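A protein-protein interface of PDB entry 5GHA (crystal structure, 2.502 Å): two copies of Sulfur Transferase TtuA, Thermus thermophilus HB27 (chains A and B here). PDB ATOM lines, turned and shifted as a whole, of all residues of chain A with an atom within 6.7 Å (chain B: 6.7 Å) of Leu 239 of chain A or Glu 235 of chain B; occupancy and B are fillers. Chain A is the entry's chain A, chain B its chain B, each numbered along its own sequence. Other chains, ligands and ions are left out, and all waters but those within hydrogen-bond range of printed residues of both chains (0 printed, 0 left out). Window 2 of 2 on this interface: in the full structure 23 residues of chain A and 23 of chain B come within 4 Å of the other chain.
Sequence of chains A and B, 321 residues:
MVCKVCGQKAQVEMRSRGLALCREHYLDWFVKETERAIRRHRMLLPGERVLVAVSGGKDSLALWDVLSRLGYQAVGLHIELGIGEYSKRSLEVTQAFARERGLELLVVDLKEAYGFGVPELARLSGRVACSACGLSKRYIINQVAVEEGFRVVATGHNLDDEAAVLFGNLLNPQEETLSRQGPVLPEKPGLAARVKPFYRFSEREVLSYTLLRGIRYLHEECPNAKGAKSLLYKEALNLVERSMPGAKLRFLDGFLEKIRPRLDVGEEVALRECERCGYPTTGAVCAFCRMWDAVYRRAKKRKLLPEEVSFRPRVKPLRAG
The side-chain sulfur (SD) of Met 244 of chain A lies within hydrogen-bond range of the side-chain hydroxyl (OH) of Tyr 233 of chain B (3.8 Å).
Among the printed residues, merely in contact across the chains: Leu 239 of chain A with Glu 235 of chain B, Ala 236 of chain A with Ala 236 of chain B, Met 244 of chain A with Leu 232 of chain B, Leu 239 of chain A with Leu 232 of chain B, Glu 235 of chain A with Leu 239 of chain B, Val 240 of chain A with Ala 236 of chain B, Ala 236 of chain A with Val 240 of chain B, Leu 239 of chain A with Leu 239 of chain B and Ser 243 of chain A with Leu 232 of chain B.
Leu 239 of chain A touches three residues of chain B. Glu 235 of chain B touches just one residue of chain A: Leu 239. Of the printed residues of chain A, Val 240 of chain B touches Ala 236. Of the printed residues of chain B, Ser 243 of chain A touches Leu 232. The nearest residue of chain A that does not touch Glu 235 of chain B is Arg 242 of chain A (5.2 Å).
Of the 11 printed residues of chain B, 6 touch a printed residue of chain A. Printed residues of chain B that touch a printed residue of chain A: Leu 232, Tyr 233, Glu 235, Ala 236, Leu 239 and Val 240. Hydrophobic or aromatic side chains of chain B that line the printed part of chain A: Leu 232, Tyr 233, Ala 236, Leu 239 and Val 240. Along chain B the printed residues that touch a printed residue of chain A span positions 232 to 240. Hydrophobic or aromatic side chains of chain A that line the printed part of chain B: Ala 236, Leu 239, Val 240 and Met 244. Among the printed residues, no Asp or Glu carboxylate lies within 4 Å of a Lys or Arg side-chain nitrogen of the other chain.
Glu 235 of chain A touches Leu 239 of chain B, and with the chains exchanged Leu 239 of chain A touches Glu 235 of chain B. Ala 236 of chain B touches its own counterpart, Ala 236 of chain A. Ala 236 of chain A touches Val 240 of chain B, and with the chains exchanged Val 240 of chain A touches Ala 236 of chain B. Leu 239 of chain B touches its own counterpart, Leu 239 of chain A. Positions printed for both chains: 234, 235, 236, 237, 238, 239 and 240.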
ATOM      1  N   LYS A 234     -31.860 -12.672 -16.185  1.00  0.00           N
ATOM      2  CA  LYS A 234     -31.927 -12.034 -14.874  1.00  0.00           C
ATOM      3  C   LYS A 234     -32.420 -12.996 -13.798  1.00  0.00           C
ATOM      4  O   LYS A 234     -31.896 -13.014 -12.684  1.00  0.00           O
ATOM      5  CB  LYS A 234     -32.840 -10.808 -14.919  1.00  0.00           C
ATOM      6  CG  LYS A 234     -32.230  -9.589 -15.582  1.00  0.00           C
ATOM      7  CD  LYS A 234     -33.228  -8.441 -15.609  1.00  0.00           C
ATOM      8  CE  LYS A 234     -32.651  -7.212 -16.287  1.00  0.00           C
ATOM      9  NZ  LYS A 234     -33.676  -6.144 -16.447  1.00  0.00           N
ATOM     10  N   GLU A 235     -33.430 -13.790 -14.135  1.00  0.00           N
ATOM     11  CA  GLU A 235     -33.999 -14.752 -13.197  1.00  0.00           C
ATOM     12  C   GLU A 235     -32.972 -15.799 -12.771  1.00  0.00           C
ATOM     13  O   GLU A 235     -32.868 -16.137 -11.593  1.00  0.00           O
ATOM     14  CB  GLU A 235     -35.221 -15.440 -13.812  1.00  0.00           C
ATOM     15  CG  GLU A 235     -35.872 -16.470 -12.905  1.00  0.00           C
ATOM     16  CD  GLU A 235     -37.155 -17.036 -13.485  1.00  0.00           C
ATOM     17  OE1 GLU A 235     -37.508 -16.676 -14.629  1.00  0.00           O
ATOM     18  OE2 GLU A 235     -37.811 -17.843 -12.793  1.00  0.00           O
ATOM     19  N   ALA A 236     -32.214 -16.303 -13.738  1.00  0.00           N
ATOM     20  CA  ALA A 236     -31.201 -17.313 -13.467  1.00  0.00           C
ATOM     21  C   ALA A 236     -30.099 -16.756 -12.572  1.00  0.00           C
ATOM     22  O   ALA A 236     -29.648 -17.423 -11.640  1.00  0.00           O
ATOM     23  CB  ALA A 236     -30.615 -17.839 -14.769  1.00  0.00           C
ATOM     24  N   LEU A 237     -29.679 -15.526 -12.856  1.00  0.00           N
ATOM     25  CA  LEU A 237     -28.610 -14.884 -12.099  1.00  0.00           C
ATOM     26  C   LEU A 237     -29.068 -14.492 -10.701  1.00  0.00           C
ATOM     27  O   LEU A 237     -28.321 -14.636  -9.735  1.00  0.00           O
ATOM     28  CB  LEU A 237     -28.089 -13.652 -12.844  1.00  0.00           C
ATOM     29  CG  LEU A 237     -27.319 -13.960 -14.126  1.00  0.00           C
ATOM     30  CD1 LEU A 237     -26.975 -12.683 -14.879  1.00  0.00           C
ATOM     31  CD2 LEU A 237     -26.064 -14.758 -13.808  1.00  0.00           C
ATOM     32  N   ASN A 238     -30.296 -13.995 -10.595  1.00  0.00           N
ATOM     33  CA  ASN A 238     -30.838 -13.605  -9.301  1.00  0.00           C
ATOM     34  C   ASN A 238     -31.106 -14.815  -8.417  1.00  0.00           C
ATOM     35  O   ASN A 238     -31.081 -14.712  -7.190  1.00  0.00           O
ATOM     36  CB  ASN A 238     -32.113 -12.782  -9.478  1.00  0.00           C
ATOM     37  CG  ASN A 238     -31.826 -11.364  -9.918  1.00  0.00           C
ATOM     38  OD1 ASN A 238     -30.836 -10.762  -9.497  1.00  0.00           O
ATOM     39  ND2 ASN A 238     -32.686 -10.821 -10.772  1.00  0.00           N
ATOM     40  N   LEU A 239     -31.359 -15.959  -9.044  1.00  0.00           N
ATOM     41  CA  LEU A 239     -31.460 -17.215  -8.313  1.00  0.00           C
ATOM     42  C   LEU A 239     -30.118 -17.534  -7.668  1.00  0.00           C
ATOM     43  O   LEU A 239     -30.056 -18.012  -6.535  1.00  0.00           O
ATOM     44  CB  LEU A 239     -31.896 -18.351  -9.238  1.00  0.00           C
ATOM     45  CG  LEU A 239     -31.968 -19.741  -8.601  1.00  0.00           C
ATOM     46  CD1 LEU A 239     -32.858 -19.724  -7.366  1.00  0.00           C
ATOM     47  CD2 LEU A 239     -32.469 -20.763  -9.608  1.00  0.00           C
ATOM     48  N   VAL A 240     -29.040 -17.258  -8.395  1.00  0.00           N
ATOM     49  CA  VAL A 240     -27.696 -17.403  -7.854  1.00  0.00           C
ATOM     50  C   VAL A 240     -27.444 -16.352  -6.776  1.00  0.00           C
ATOM     51  O   VAL A 240     -26.922 -16.659  -5.702  1.00  0.00           O
ATOM     52  CB  VAL A 240     -26.623 -17.273  -8.956  1.00  0.00           C
ATOM     53  CG1 VAL A 240     -25.226 -17.365  -8.358  1.00  0.00           C
ATOM     54  CG2 VAL A 240     -26.826 -18.334 -10.026  1.00  0.00           C
ATOM     55  N   GLU A 241     -27.834 -15.116  -7.071  1.00  0.00           N
ATOM     56  CA  GLU A 241     -27.615 -13.984  -6.173  1.00  0.00           C
ATOM     57  C   GLU A 241     -28.243 -14.194  -4.796  1.00  0.00           C
ATOM     58  O   GLU A 241     -27.663 -13.818  -3.778  1.00  0.00           O
ATOM     59  CB  GLU A 241     -28.168 -12.702  -6.801  1.00  0.00           C
ATOM     60  CG  GLU A 241     -27.956 -11.450  -5.965  1.00  0.00           C
ATOM     61  CD  GLU A 241     -26.503 -11.022  -5.903  1.00  0.00           C
ATOM     62  OE1 GLU A 241     -25.718 -11.420  -6.791  1.00  0.00           O
ATOM     63  OE2 GLU A 241     -26.143 -10.281  -4.965  1.00  0.00           O
ATOM     64  N   ARG A 242     -29.429 -14.795  -4.776  1.00  0.00           N
ATOM     65  CA  ARG A 242     -30.153 -15.045  -3.535  1.00  0.00           C
ATOM     66  C   ARG A 242     -29.355 -15.910  -2.557  1.00  0.00           C
ATOM     67  O   ARG A 242     -29.366 -15.666  -1.352  1.00  0.00           O
ATOM     68  CB  ARG A 242     -31.499 -15.708  -3.834  1.00  0.00           C
ATOM     69  CG  ARG A 242     -32.345 -15.988  -2.602  1.00  0.00           C
ATOM     70  CD  ARG A 242     -33.655 -16.660  -2.977  1.00  0.00           C
ATOM     71  NE  ARG A 242     -33.432 -17.919  -3.680  1.00  0.00           N
ATOM     72  CZ  ARG A 242     -33.430 -19.113  -3.096  1.00  0.00           C
ATOM     73  NH1 ARG A 242     -33.216 -20.205  -3.818  1.00  0.00           N
ATOM     74  NH2 ARG A 242     -33.647 -19.219  -1.791  1.00  0.00           N
ATOM     75  N   SER A 243     -28.657 -16.910  -3.085  1.00  0.00           N
ATOM     76  CA  SER A 243     -27.906 -17.847  -2.255  1.00  0.00           C
ATOM     77  C   SER A 243     -26.432 -17.468  -2.139  1.00  0.00           C
ATOM     78  O   SER A 243     -25.740 -17.908  -1.219  1.00  0.00           O
ATOM     79  CB  SER A 243     -28.037 -19.265  -2.814  1.00  0.00           C
ATOM     80  OG  SER A 243     -29.400 -19.642  -2.903  1.00  0.00           O
ATOM     81  N   MET A 244     -25.953 -16.660  -3.080  1.00  0.00           N
ATOM     82  CA  MET A 244     -24.570 -16.193  -3.058  1.00  0.00           C
ATOM     83  C   MET A 244     -24.500 -14.694  -3.307  1.00  0.00           C
ATOM     84  O   MET A 244     -24.233 -14.265  -4.427  1.00  0.00           O
ATOM     85  CB  MET A 244     -23.731 -16.935  -4.100  1.00  0.00           C
ATOM     86  CG  MET A 244     -23.566 -18.421  -3.829  1.00  0.00           C
ATOM     87  SD  MET A 244     -22.453 -19.219  -5.001  1.00  0.00           S
ATOM     88  CE  MET A 244     -20.935 -18.326  -4.683  1.00  0.00           C
ATOM     89  N   SER B 230     -22.314 -26.362  -6.879  1.00  0.00           N
ATOM     90  CA  SER B 230     -22.621 -26.892  -8.201  1.00  0.00           C
ATOM     91  C   SER B 230     -24.116 -27.138  -8.370  1.00  0.00           C
ATOM     92  O   SER B 230     -24.649 -27.014  -9.470  1.00  0.00           O
ATOM     93  CB  SER B 230     -21.840 -28.183  -8.455  1.00  0.00           C
ATOM     94  OG  SER B 230     -22.154 -29.167  -7.486  1.00  0.00           O
ATOM     95  N   LEU B 231     -24.790 -27.483  -7.276  1.00  0.00           N
ATOM     96  CA  LEU B 231     -26.240 -27.637  -7.295  1.00  0.00           C
ATOM     97  C   LEU B 231     -26.915 -26.322  -7.656  1.00  0.00           C
ATOM     98  O   LEU B 231     -27.811 -26.283  -8.501  1.00  0.00           O
ATOM     99  CB  LEU B 231     -26.755 -28.134  -5.943  1.00  0.00           C
ATOM    100  CG  LEU B 231     -26.448 -29.595  -5.616  1.00  0.00           C
ATOM    101  CD1 LEU B 231     -27.120 -30.013  -4.316  1.00  0.00           C
ATOM    102  CD2 LEU B 231     -26.890 -30.478  -6.763  1.00  0.00           C
ATOM    103  N   LEU B 232     -26.476 -25.248  -7.005  1.00  0.00           N
ATOM    104  CA  LEU B 232     -26.970 -23.910  -7.297  1.00  0.00           C
ATOM    105  C   LEU B 232     -26.697 -23.544  -8.751  1.00  0.00           C
ATOM    106  O   LEU B 232     -27.570 -23.017  -9.446  1.00  0.00           O
ATOM    107  CB  LEU B 232     -26.321 -22.885  -6.363  1.00  0.00           C
ATOM    108  CG  LEU B 232     -26.693 -21.420  -6.595  1.00  0.00           C
ATOM    109  CD1 LEU B 232     -28.151 -21.170  -6.240  1.00  0.00           C
ATOM    110  CD2 LEU B 232     -25.777 -20.503  -5.807  1.00  0.00           C
ATOM    111  N   TYR B 233     -25.482 -23.837  -9.203  1.00  0.00           N
ATOM    112  CA  TYR B 233     -25.070 -23.543 -10.569  1.00  0.00           C
ATOM    113  C   TYR B 233     -25.910 -24.309 -11.586  1.00  0.00           C
ATOM    114  O   TYR B 233     -26.355 -23.745 -12.588  1.00  0.00           O
ATOM    115  CB  TYR B 233     -23.590 -23.877 -10.763  1.00  0.00           C
ATOM    116  CG  TYR B 233     -22.659 -23.128  -9.838  1.00  0.00           C
ATOM    117  CD1 TYR B 233     -23.013 -21.892  -9.310  1.00  0.00           C
ATOM    118  CD2 TYR B 233     -21.422 -23.658  -9.494  1.00  0.00           C
ATOM    119  CE1 TYR B 233     -22.160 -21.206  -8.465  1.00  0.00           C
ATOM    120  CE2 TYR B 233     -20.564 -22.983  -8.650  1.00  0.00           C
ATOM    121  CZ  TYR B 233     -20.936 -21.756  -8.139  1.00  0.00           C
ATOM    122  OH  TYR B 233     -20.078 -21.083  -7.300  1.00  0.00           O
ATOM    123  N   LYS B 234     -26.119 -25.596 -11.321  1.00  0.00           N
ATOM    124  CA  LYS B 234     -26.911 -26.446 -12.202  1.00  0.00           C
ATOM    125  C   LYS B 234     -28.359 -25.976 -12.291  1.00  0.00           C
ATOM    126  O   LYS B 234     -28.965 -26.016 -13.361  1.00  0.00           O
ATOM    127  CB  LYS B 234     -26.868 -27.900 -11.730  1.00  0.00           C
ATOM    128  CG  LYS B 234     -25.554 -28.611 -12.000  1.00  0.00           C
ATOM    129  CD  LYS B 234     -25.632 -30.066 -11.584  1.00  0.00           C
ATOM    130  CE  LYS B 234     -24.331 -30.785 -11.866  1.00  0.00           C
ATOM    131  NZ  LYS B 234     -24.424 -32.236 -11.540  1.00  0.00           N
ATOM    132  N   GLU B 235     -28.909 -25.525 -11.168  1.00  0.00           N
ATOM    133  CA  GLU B 235     -30.306 -25.114 -11.131  1.00  0.00           C
ATOM    134  C   GLU B 235     -30.552 -23.867 -11.982  1.00  0.00           C
ATOM    135  O   GLU B 235     -31.592 -23.746 -12.627  1.00  0.00           O
ATOM    136  CB  GLU B 235     -30.761 -24.859  -9.693  1.00  0.00           C
ATOM    137  CG  GLU B 235     -32.273 -24.841  -9.550  1.00  0.00           C
ATOM    138  CD  GLU B 235     -32.755 -23.988  -8.396  1.00  0.00           C
ATOM    139  OE1 GLU B 235     -31.981 -23.779  -7.438  1.00  0.00           O
ATOM    140  OE2 GLU B 235     -33.914 -23.519  -8.455  1.00  0.00           O
ATOM    141  N   ALA B 236     -29.597 -22.943 -11.975  1.00  0.00           N
ATOM    142  CA  ALA B 236     -29.721 -21.718 -12.762  1.00  0.00           C
ATOM    143  C   ALA B 236     -29.589 -22.006 -14.256  1.00  0.00           C
ATOM    144  O   ALA B 236     -30.360 -21.491 -15.066  1.00  0.00           O
ATOM    145  CB  ALA B 236     -28.681 -20.698 -12.323  1.00  0.00           C
ATOM    146  N   LEU B 237     -28.610 -22.835 -14.613  1.00  0.00           N
ATOM    147  CA  LEU B 237     -28.392 -23.220 -16.005  1.00  0.00           C
ATOM    148  C   LEU B 237     -29.568 -24.022 -16.556  1.00  0.00           C
ATOM    149  O   LEU B 237     -29.930 -23.892 -17.726  1.00  0.00           O
ATOM    150  CB  LEU B 237     -27.100 -24.028 -16.143  1.00  0.00           C
ATOM    151  CG  LEU B 237     -25.780 -23.318 -15.838  1.00  0.00           C
ATOM    152  CD1 LEU B 237     -24.622 -24.307 -15.840  1.00  0.00           C
ATOM    153  CD2 LEU B 237     -25.531 -22.205 -16.840  1.00  0.00           C
ATOM    154  N   ASN B 238     -30.158 -24.858 -15.707  1.00  0.00           N
ATOM    155  CA  ASN B 238     -31.304 -25.663 -16.110  1.00  0.00           C
ATOM    156  C   ASN B 238     -32.591 -24.845 -16.147  1.00  0.00           C
ATOM    157  O   ASN B 238     -33.537 -25.194 -16.853  1.00  0.00           O
ATOM    158  CB  ASN B 238     -31.466 -26.863 -15.179  1.00  0.00           C
ATOM    159  CG  ASN B 238     -30.521 -27.998 -15.525  1.00  0.00           C
ATOM    160  OD1 ASN B 238     -30.413 -28.401 -16.685  1.00  0.00           O
ATOM    161  ND2 ASN B 238     -29.824 -28.515 -14.520  1.00  0.00           N
ATOM    162  N   LEU B 239     -32.624 -23.759 -15.385  1.00  0.00           N
ATOM    163  CA  LEU B 239     -33.754 -22.842 -15.433  1.00  0.00           C
ATOM    164  C   LEU B 239     -33.797 -22.196 -16.814  1.00  0.00           C
ATOM    165  O   LEU B 239     -34.869 -21.980 -17.379  1.00  0.00           O
ATOM    166  CB  LEU B 239     -33.647 -21.787 -14.331  1.00  0.00           C
ATOM    167  CG  LEU B 239     -34.872 -20.913 -14.046  1.00  0.00           C
ATOM    168  CD1 LEU B 239     -34.934 -20.565 -12.570  1.00  0.00           C
ATOM    169  CD2 LEU B 239     -34.841 -19.643 -14.875  1.00  0.00           C
ATOM    170  N   VAL B 240     -32.618 -21.901 -17.351  1.00  0.00           N
ATOM    171  CA  VAL B 240     -32.493 -21.377 -18.705  1.00  0.00           C
ATOM    172  C   VAL B 240     -32.847 -22.437 -19.737  1.00  0.00           C
ATOM    173  O   VAL B 240     -33.611 -22.177 -20.666  1.00  0.00           O
ATOM    174  CB  VAL B 240     -31.066 -20.864 -18.980  1.00  0.00           C
ATOM    175  CG1 VAL B 240     -30.852 -20.653 -20.471  1.00  0.00           C
ATOM    176  CG2 VAL B 240     -30.799 -19.582 -18.202  1.00  0.00           C
